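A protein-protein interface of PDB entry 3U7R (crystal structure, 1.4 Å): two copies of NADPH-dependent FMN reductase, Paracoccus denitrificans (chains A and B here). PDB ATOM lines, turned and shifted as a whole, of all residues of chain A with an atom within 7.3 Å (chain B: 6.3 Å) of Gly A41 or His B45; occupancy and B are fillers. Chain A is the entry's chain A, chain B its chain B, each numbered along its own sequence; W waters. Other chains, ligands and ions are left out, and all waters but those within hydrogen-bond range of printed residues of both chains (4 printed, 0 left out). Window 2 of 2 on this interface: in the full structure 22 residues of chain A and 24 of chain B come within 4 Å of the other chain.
O of Leu A43 is in hydrogen-bond range of NE2 of His B45 (2.9 Å).
The backbone carbonyl oxygen of Leu B43 lies within hydrogen-bond range of a ring nitrogen (NE2) of His A45.
O of Pro A44 lies within hydrogen-bond range of ND2 of Asn A88 (2.9 Å).
N of Tyr A46 sits at hydrogen-bond distance from OD1 of Asn A88 (2.8 Å).
The backbone carbonyl oxygen (O) of Pro B44 sits at hydrogen-bond distance from the side-chain amide nitrogen (ND2) of Asn B88, at 2.9 Å.
N of Tyr B46 is in hydrogen-bond range of OD1 of Asn B88 (2.8 Å).
CB of Leu A12 touches ND2 of Asn B47, 3.7 Å away.
His B45 touches Ile A40 (NE2 to O, 3.8 Å).
Gly A41 touches His B45 (O to CD2, 3.4 Å).
His A45 touches Asn B88.
ND1 of His B45 touches CG of Met A85, at 3.8 Å.
ND2 of Asn A88 touches CE1 of His B45, 3.8 Å away.
Of chain B, only His B45 comes within 4 Å of Gly A41.
His B45 touches five residues of chain A.
Printed residues of chain A within 4 Å of Asn B47: Leu A12.
Printed residues of chain A within 4 Å of Asn B88: His A45 (3.8 Å).
Printed residues of chain B within 4 Å of Ile A40: His B45 (3.8 Å).
Printed residues of chain A within 4 Å of Leu B43: His A45 (2.8 Å).
Val A9 touches none of the printed residues of chain B.
Printed residues of chain B that touch a printed residue of chain A: Leu B43, His B45, Asn B47 and Asn B88.
Hydrophobic or aromatic side chains of chain B that line the printed part of chain A: His B45.
Of the 18 printed residues of chain A, 7 touch a printed residue of chain B.
Hydrophobic or aromatic side chains of chain A that line the printed part of chain B: Leu A12, His A45 and Met A85.
Among the printed residues, 8 pairs touch across the chains.
Leu A43 touches His B45, and with the chains exchanged His A45 touches Leu B43.
His A45 touches Asn B88, and with the chains exchanged Asn A88 touches His B45.
Of the 8 pairs that touch across the chains among the printed residues, 4 have their exchanged pair printed and touching as well.
Water W2 bridges the backbone carbonyl oxygen (O) of Tyr B46 (2.7 Å) and the backbone NH (N) of Leu A12 (2.9 Å).
Water W3 bridges the backbone NH of Gly A84 (2.7 Å) and the backbone NH of Asn B88 (3.4 Å).
Water W1 lies within hydrogen-bond range of the side-chain amide oxygen of Asn B88 (2.8 Å) and the backbone NH of Met A85 (3.0 Å).
Water W4 lies within hydrogen-bond range of a ring nitrogen (ND1) of His B45, the backbone NH (N) of Met A85 and the side-chain amide oxygen (OD1) of Asn B88.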
ATOM      1  N   VAL A   9      -1.457   8.581 -34.434  1.00  0.00           N
ATOM      2  CA  VAL A   9      -2.846   8.637 -34.045  1.00  0.00           C
ATOM      3  C   VAL A   9      -2.928   9.544 -32.841  1.00  0.00           C
ATOM      4  O   VAL A   9      -2.346   9.267 -31.783  1.00  0.00           O
ATOM      5  CB  VAL A   9      -3.400   7.240 -33.719  1.00  0.00           C
ATOM      6  CG1 VAL A   9      -4.866   7.359 -33.255  1.00  0.00           C
ATOM      7  CG2 VAL A   9      -3.294   6.286 -34.906  1.00  0.00           C
ATOM      8  N   LEU A  12      -4.944   8.692 -27.155  1.00  0.00           N
ATOM      9  CA  LEU A  12      -4.460   7.593 -26.320  1.00  0.00           C
ATOM     10  C   LEU A  12      -5.602   6.804 -25.681  1.00  0.00           C
ATOM     11  O   LEU A  12      -5.341   5.751 -25.070  1.00  0.00           O
ATOM     12  CB  LEU A  12      -3.544   8.108 -25.207  1.00  0.00           C
ATOM     13  CG  LEU A  12      -2.323   8.912 -25.652  1.00  0.00           C
ATOM     14  CD1 LEU A  12      -1.550   9.330 -24.410  1.00  0.00           C
ATOM     15  CD2 LEU A  12      -1.474   8.092 -26.597  1.00  0.00           C
ATOM     16  N   LEU A  38       3.723   5.268 -34.743  1.00  0.00           N
ATOM     17  CA  LEU A  38       4.669   6.064 -33.998  1.00  0.00           C
ATOM     18  C   LEU A  38       4.123   6.221 -32.601  1.00  0.00           C
ATOM     19  O   LEU A  38       2.976   6.629 -32.419  1.00  0.00           O
ATOM     20  CB  LEU A  38       4.850   7.425 -34.655  1.00  0.00           C
ATOM     21  CG  LEU A  38       5.431   7.399 -36.062  1.00  0.00           C
ATOM     22  CD1 LEU A  38       5.421   8.782 -36.680  1.00  0.00           C
ATOM     23  CD2 LEU A  38       6.828   6.799 -36.050  1.00  0.00           C
ATOM     24  N   HIS A  39       4.961   5.940 -31.632  1.00  0.00           N
ATOM     25  CA  HIS A  39       4.525   5.916 -30.239  1.00  0.00           C
ATOM     26  C   HIS A  39       4.636   7.267 -29.580  1.00  0.00           C
ATOM     27  O   HIS A  39       5.483   7.513 -28.739  1.00  0.00           O
ATOM     28  CB  HIS A  39       5.337   4.847 -29.526  1.00  0.00           C
ATOM     29  CG  HIS A  39       5.208   3.517 -30.190  1.00  0.00           C
ATOM     30  ND1 HIS A  39       4.019   2.845 -30.220  1.00  0.00           N
ATOM     31  CD2 HIS A  39       6.098   2.745 -30.851  1.00  0.00           C
ATOM     32  CE1 HIS A  39       4.172   1.714 -30.891  1.00  0.00           C
ATOM     33  NE2 HIS A  39       5.422   1.632 -31.279  1.00  0.00           N
ATOM     34  N   ILE A  40       3.756   8.156 -29.992  1.00  0.00           N
ATOM     35  CA  ILE A  40       3.852   9.542 -29.588  1.00  0.00           C
ATOM     36  C   ILE A  40       3.471   9.772 -28.133  1.00  0.00           C
ATOM     37  O   ILE A  40       3.953  10.714 -27.519  1.00  0.00           O
ATOM     38  CB  ILE A  40       3.064  10.468 -30.535  1.00  0.00           C
ATOM     39  CG1 ILE A  40       1.541  10.232 -30.507  1.00  0.00           C
ATOM     40  CG2 ILE A  40       3.579  10.333 -31.985  1.00  0.00           C
ATOM     41  CD1 ILE A  40       0.797  11.258 -31.337  1.00  0.00           C
ATOM     42  N   GLY A  41       2.662   8.899 -27.559  1.00  0.00           N
ATOM     43  CA  GLY A  41       2.335   8.995 -26.137  1.00  0.00           C
ATOM     44  C   GLY A  41       3.514   8.649 -25.229  1.00  0.00           C
ATOM     45  O   GLY A  41       3.510   9.012 -24.051  1.00  0.00           O
ATOM     46  N   ASP A  42       4.539   8.002 -25.780  1.00  0.00           N
ATOM     47  CA  ASP A  42       5.718   7.595 -25.013  1.00  0.00           C
ATOM     48  C   ASP A  42       6.816   8.644 -25.016  1.00  0.00           C
ATOM     49  O   ASP A  42       7.848   8.436 -24.392  1.00  0.00           O
ATOM     50  CB  ASP A  42       6.257   6.288 -25.612  1.00  0.00           C
ATOM     51  CG  ASP A  42       5.227   5.181 -25.495  1.00  0.00           C
ATOM     52  OD1 ASP A  42       5.138   4.550 -24.435  1.00  0.00           O
ATOM     53  OD2 ASP A  42       4.383   5.061 -26.421  1.00  0.00           O
ATOM     54  N   LEU A  43       6.604   9.761 -25.709  1.00  0.00           N
ATOM     55  CA  LEU A  43       7.592  10.836 -25.781  1.00  0.00           C
ATOM     56  C   LEU A  43       7.432  11.747 -24.598  1.00  0.00           C
ATOM     57  O   LEU A  43       6.318  12.162 -24.301  1.00  0.00           O
ATOM     58  CB  LEU A  43       7.390  11.688 -27.034  1.00  0.00           C
ATOM     59  CG  LEU A  43       7.506  10.871 -28.327  1.00  0.00           C
ATOM     60  CD1 LEU A  43       7.066  11.687 -29.514  1.00  0.00           C
ATOM     61  CD2 LEU A  43       8.925  10.363 -28.547  1.00  0.00           C
ATOM     62  N   PRO A  44       8.520  12.140 -23.968  1.00  0.00           N
ATOM     63  CA  PRO A  44       8.415  13.161 -22.923  1.00  0.00           C
ATOM     64  C   PRO A  44       8.101  14.516 -23.576  1.00  0.00           C
ATOM     65  O   PRO A  44       8.253  14.675 -24.789  1.00  0.00           O
ATOM     66  CB  PRO A  44       9.820  13.162 -22.305  1.00  0.00           C
ATOM     67  CG  PRO A  44      10.707  12.755 -23.415  1.00  0.00           C
ATOM     68  CD  PRO A  44       9.914  11.734 -24.213  1.00  0.00           C
ATOM     69  N   HIS A  45       7.676  15.485 -22.784  1.00  0.00           N
ATOM     70  CA  HIS A  45       7.594  16.847 -23.294  1.00  0.00           C
ATOM     71  C   HIS A  45       8.930  17.246 -23.830  1.00  0.00           C
ATOM     72  O   HIS A  45       9.988  17.022 -23.209  1.00  0.00           O
ATOM     73  CB  HIS A  45       7.163  17.808 -22.221  1.00  0.00           C
ATOM     74  CG  HIS A  45       5.754  17.636 -21.762  1.00  0.00           C
ATOM     75  ND1 HIS A  45       4.664  17.622 -22.600  1.00  0.00           N
ATOM     76  CD2 HIS A  45       5.258  17.506 -20.504  1.00  0.00           C
ATOM     77  CE1 HIS A  45       3.563  17.450 -21.890  1.00  0.00           C
ATOM     78  NE2 HIS A  45       3.896  17.404 -20.616  1.00  0.00           N
ATOM     79  N   TYR A  46       8.902  17.933 -24.968  1.00  0.00           N
ATOM     80  CA  TYR A  46      10.160  18.356 -25.605  1.00  0.00           C
ATOM     81  C   TYR A  46      11.005  19.112 -24.571  1.00  0.00           C
ATOM     82  O   TYR A  46      10.502  19.993 -23.874  1.00  0.00           O
ATOM     83  CB  TYR A  46       9.948  19.270 -26.848  1.00  0.00           C
ATOM     84  CG  TYR A  46      11.239  19.416 -27.578  1.00  0.00           C
ATOM     85  CD1 TYR A  46      11.608  18.548 -28.612  1.00  0.00           C
ATOM     86  CD2 TYR A  46      12.151  20.384 -27.184  1.00  0.00           C
ATOM     87  CE1 TYR A  46      12.856  18.610 -29.188  1.00  0.00           C
ATOM     88  CE2 TYR A  46      13.396  20.434 -27.766  1.00  0.00           C
ATOM     89  CZ  TYR A  46      13.739  19.550 -28.761  1.00  0.00           C
ATOM     90  OH  TYR A  46      15.026  19.572 -29.326  1.00  0.00           O
ATOM     91  N   SER A  57      12.524   6.599 -26.671  1.00  0.00           N
ATOM     92  CA  SER A  57      11.302   6.817 -27.429  1.00  0.00           C
ATOM     93  C   SER A  57      11.522   7.778 -28.582  1.00  0.00           C
ATOM     94  O   SER A  57      10.913   7.623 -29.644  1.00  0.00           O
ATOM     95  CB  SER A  57      10.186   7.337 -26.523  1.00  0.00           C
ATOM     96  OG  SER A  57      10.594   8.549 -25.938  1.00  0.00           O
ATOM     97  N   GLY A  84      -1.667  18.798 -28.771  1.00  0.00           N
ATOM     98  CA  GLY A  84      -0.267  19.098 -28.524  1.00  0.00           C
ATOM     99  C   GLY A  84       0.633  17.894 -28.550  1.00  0.00           C
ATOM    100  O   GLY A  84       1.795  18.013 -28.971  1.00  0.00           O
ATOM    101  N   MET A  85       0.133  16.710 -28.169  1.00  0.00           N
ATOM    102  CA  MET A  85       0.991  15.540 -28.223  1.00  0.00           C
ATOM    103  C   MET A  85       1.493  15.283 -29.640  1.00  0.00           C
ATOM    104  O   MET A  85       2.587  14.766 -29.826  1.00  0.00           O
ATOM    105  CB  MET A  85       0.131  14.385 -27.713  1.00  0.00           C
ATOM    106  CG  MET A  85       0.857  13.059 -27.750  1.00  0.00           C
ATOM    107  SD  MET A  85      -0.245  11.562 -27.089  1.00  0.00           S
ATOM    108  CE  MET A  85      -1.623  11.557 -28.460  1.00  0.00           C
ATOM    109  N   ILE A  86       0.691  15.595 -30.663  1.00  0.00           N
ATOM    110  CA  ILE A  86       1.198  15.424 -32.037  1.00  0.00           C
ATOM    111  C   ILE A  86       2.295  16.445 -32.337  1.00  0.00           C
ATOM    112  O   ILE A  86       3.325  16.095 -32.891  1.00  0.00           O
ATOM    113  CB  ILE A  86       0.076  15.514 -33.086  1.00  0.00           C
ATOM    114  CG1 ILE A  86      -0.865  14.318 -32.952  1.00  0.00           C
ATOM    115  CG2 ILE A  86       0.645  15.652 -34.483  1.00  0.00           C
ATOM    116  CD1 ILE A  86      -2.037  14.349 -33.902  1.00  0.00           C
ATOM    117  N   ASN A  88       4.283  17.843 -30.281  1.00  0.00           N
ATOM    118  CA  ASN A  88       5.465  17.419 -29.527  1.00  0.00           C
ATOM    119  C   ASN A  88       6.257  16.390 -30.288  1.00  0.00           C
ATOM    120  O   ASN A  88       7.489  16.473 -30.366  1.00  0.00           O
ATOM    121  CB  ASN A  88       4.969  16.895 -28.201  1.00  0.00           C
ATOM    122  CG  ASN A  88       6.089  16.647 -27.215  1.00  0.00           C
ATOM    123  OD1 ASN A  88       6.798  17.579 -26.774  1.00  0.00           O
ATOM    124  ND2 ASN A  88       6.221  15.370 -26.783  1.00  0.00           N
ATOM    125  N   ALA A  89       5.566  15.419 -30.910  1.00  0.00           N
ATOM    126  CA  ALA A  89       6.235  14.427 -31.753  1.00  0.00           C
ATOM    127  C   ALA A  89       6.892  15.026 -32.999  1.00  0.00           C
ATOM    128  O   ALA A  89       8.020  14.709 -33.369  1.00  0.00           O
ATOM    129  CB  ALA A  89       5.249  13.328 -32.152  1.00  0.00           C
ATOM    130  N   TRP A  92      10.091  16.842 -31.747  1.00  0.00           N
ATOM    131  CA  TRP A  92      11.167  15.904 -31.423  1.00  0.00           C
ATOM    132  C   TRP A  92      11.855  15.416 -32.687  1.00  0.00           C
ATOM    133  O   TRP A  92      13.099  15.336 -32.752  1.00  0.00           O
ATOM    134  CB  TRP A  92      10.654  14.714 -30.616  1.00  0.00           C
ATOM    135  CG  TRP A  92      10.657  14.901 -29.157  1.00  0.00           C
ATOM    136  CD1 TRP A  92       9.574  14.894 -28.305  1.00  0.00           C
ATOM    137  CD2 TRP A  92      11.814  15.103 -28.336  1.00  0.00           C
ATOM    138  NE1 TRP A  92      10.007  15.074 -27.013  1.00  0.00           N
ATOM    139  CE2 TRP A  92      11.377  15.189 -26.996  1.00  0.00           C
ATOM    140  CE3 TRP A  92      13.166  15.227 -28.610  1.00  0.00           C
ATOM    141  CZ2 TRP A  92      12.252  15.406 -25.946  1.00  0.00           C
ATOM    142  CZ3 TRP A  92      14.031  15.412 -27.578  1.00  0.00           C
ATOM    143  CH2 TRP A  92      13.588  15.483 -26.250  1.00  0.00           C
ATOM    144  N   LEU B  43       2.119  18.046 -16.528  1.00  0.00           N
ATOM    145  CA  LEU B  43       0.876  17.453 -17.047  1.00  0.00           C
ATOM    146  C   LEU B  43       1.192  16.233 -17.905  1.00  0.00           C
ATOM    147  O   LEU B  43       2.077  16.335 -18.778  1.00  0.00           O
ATOM    148  CB  LEU B  43       0.136  18.472 -17.918  1.00  0.00           C
ATOM    149  CG  LEU B  43      -0.246  19.730 -17.163  1.00  0.00           C
ATOM    150  CD1 LEU B  43      -0.727  20.807 -18.105  1.00  0.00           C
ATOM    151  CD2 LEU B  43      -1.292  19.506 -16.076  1.00  0.00           C
ATOM    152  N   PRO B  44       0.451  15.126 -17.732  1.00  0.00           N
ATOM    153  CA  PRO B  44       0.577  14.038 -18.699  1.00  0.00           C
ATOM    154  C   PRO B  44       0.037  14.472 -20.053  1.00  0.00           C
ATOM    155  O   PRO B  44      -0.699  15.461 -20.152  1.00  0.00           O
ATOM    156  CB  PRO B  44      -0.272  12.944 -18.081  1.00  0.00           C
ATOM    157  CG  PRO B  44      -1.312  13.692 -17.361  1.00  0.00           C
ATOM    158  CD  PRO B  44      -0.648  14.917 -16.788  1.00  0.00           C
ATOM    159  N   HIS B  45       0.355  13.720 -21.091  1.00  0.00           N
ATOM    160  CA  HIS B  45      -0.352  13.936 -22.350  1.00  0.00           C
ATOM    161  C   HIS B  45      -1.829  13.785 -22.119  1.00  0.00           C
ATOM    162  O   HIS B  45      -2.315  12.845 -21.463  1.00  0.00           O
ATOM    163  CB  HIS B  45       0.085  12.954 -23.440  1.00  0.00           C
ATOM    164  CG  HIS B  45       1.486  13.158 -23.886  1.00  0.00           C
ATOM    165  ND1 HIS B  45       1.954  14.364 -24.351  1.00  0.00           N
ATOM    166  CD2 HIS B  45       2.528  12.299 -23.939  1.00  0.00           C
ATOM    167  CE1 HIS B  45       3.214  14.230 -24.713  1.00  0.00           C
ATOM    168  NE2 HIS B  45       3.582  12.988 -24.479  1.00  0.00           N
ATOM    169  N   TYR B  46      -2.586  14.666 -22.745  1.00  0.00           N
ATOM    170  CA  TYR B  46      -4.043  14.631 -22.609  1.00  0.00           C
ATOM    171  C   TYR B  46      -4.584  13.217 -22.897  1.00  0.00           C
ATOM    172  O   TYR B  46      -4.209  12.610 -23.891  1.00  0.00           O
ATOM    173  CB  TYR B  46      -4.812  15.630 -23.527  1.00  0.00           C
ATOM    174  CG  TYR B  46      -6.253  15.751 -23.082  1.00  0.00           C
ATOM    175  CD1 TYR B  46      -6.644  16.708 -22.148  1.00  0.00           C
ATOM    176  CD2 TYR B  46      -7.188  14.852 -23.525  1.00  0.00           C
ATOM    177  CE1 TYR B  46      -7.928  16.777 -21.703  1.00  0.00           C
ATOM    178  CE2 TYR B  46      -8.472  14.877 -23.029  1.00  0.00           C
ATOM    179  CZ  TYR B  46      -8.827  15.832 -22.107  1.00  0.00           C
ATOM    180  OH  TYR B  46     -10.121  15.816 -21.582  1.00  0.00           O
ATOM    181  N   ASN B  47      -5.415  12.708 -21.998  1.00  0.00           N
ATOM    182  CA  ASN B  47      -6.089  11.431 -22.210  1.00  0.00           C
ATOM    183  C   ASN B  47      -7.383  11.519 -21.445  1.00  0.00           C
ATOM    184  O   ASN B  47      -7.383  11.611 -20.237  1.00  0.00           O
ATOM    185  CB  ASN B  47      -5.223  10.244 -21.739  1.00  0.00           C
ATOM    186  CG  ASN B  47      -5.898   8.908 -21.956  1.00  0.00           C
ATOM    187  OD1 ASN B  47      -7.109   8.821 -22.105  1.00  0.00           O
ATOM    188  ND2 ASN B  47      -5.106   7.836 -21.904  1.00  0.00           N
ATOM    189  N   LEU B  50      -8.343   9.644 -18.199  1.00  0.00           N
ATOM    190  CA  LEU B  50      -7.764  10.017 -16.898  1.00  0.00           C
ATOM    191  C   LEU B  50      -8.683  10.839 -16.024  1.00  0.00           C
ATOM    192  O   LEU B  50      -8.416  10.975 -14.815  1.00  0.00           O
ATOM    193  CB  LEU B  50      -6.439  10.767 -17.080  1.00  0.00           C
ATOM    194  CG  LEU B  50      -5.386   9.961 -17.840  1.00  0.00           C
ATOM    195  CD1 LEU B  50      -4.167  10.836 -17.983  1.00  0.00           C
ATOM    196  CD2 LEU B  50      -5.036   8.642 -17.161  1.00  0.00           C
ATOM    197  N   ASN B  88      -1.234  21.268 -24.889  1.00  0.00           N
ATOM    198  CA  ASN B  88      -1.702  20.200 -23.967  1.00  0.00           C
ATOM    199  C   ASN B  88      -2.290  20.804 -22.697  1.00  0.00           C
ATOM    200  O   ASN B  88      -3.311  20.343 -22.206  1.00  0.00           O
ATOM    201  CB  ASN B  88      -0.481  19.338 -23.650  1.00  0.00           C
ATOM    202  CG  ASN B  88      -0.821  18.057 -22.912  1.00  0.00           C
ATOM    203  OD1 ASN B  88      -1.546  17.198 -23.424  1.00  0.00           O
ATOM    204  ND2 ASN B  88      -0.252  17.901 -21.708  1.00  0.00           N
ATOM    205  N   TRP B  92      -6.167  20.533 -21.414  1.00  0.00           N
ATOM    206  CA  TRP B  92      -6.532  20.019 -20.098  1.00  0.00           C
ATOM    207  C   TRP B  92      -7.446  20.976 -19.355  1.00  0.00           C
ATOM    208  O   TRP B  92      -8.433  20.555 -18.736  1.00  0.00           O
ATOM    209  CB  TRP B  92      -5.272  19.756 -19.250  1.00  0.00           C
ATOM    210  CG  TRP B  92      -4.695  18.390 -19.371  1.00  0.00           C
ATOM    211  CD1 TRP B  92      -3.439  18.043 -19.819  1.00  0.00           C
ATOM    212  CD2 TRP B  92      -5.331  17.162 -18.967  1.00  0.00           C
ATOM    213  NE1 TRP B  92      -3.282  16.680 -19.727  1.00  0.00           N
ATOM    214  CE2 TRP B  92      -4.421  16.124 -19.230  1.00  0.00           C
ATOM    215  CE3 TRP B  92      -6.602  16.844 -18.466  1.00  0.00           C
ATOM    216  CZ2 TRP B  92      -4.724  14.790 -18.977  1.00  0.00           C
ATOM    217  CZ3 TRP B  92      -6.893  15.531 -18.178  1.00  0.00           C
ATOM    218  CH2 TRP B  92      -5.961  14.511 -18.455  1.00  0.00           C
HETATM  219  O   HOH W   1      -2.060  16.545 -26.092  1.00  0.00           O
HETATM  220  O   HOH W   2      -5.481  11.142 -25.785  1.00  0.00           O
HETATM  221  O   HOH W   3      -3.232  19.030 -26.550  1.00  0.00           O
HETATM  222  O   HOH W   4       1.192  16.967 -25.146  1.00  0.00           O
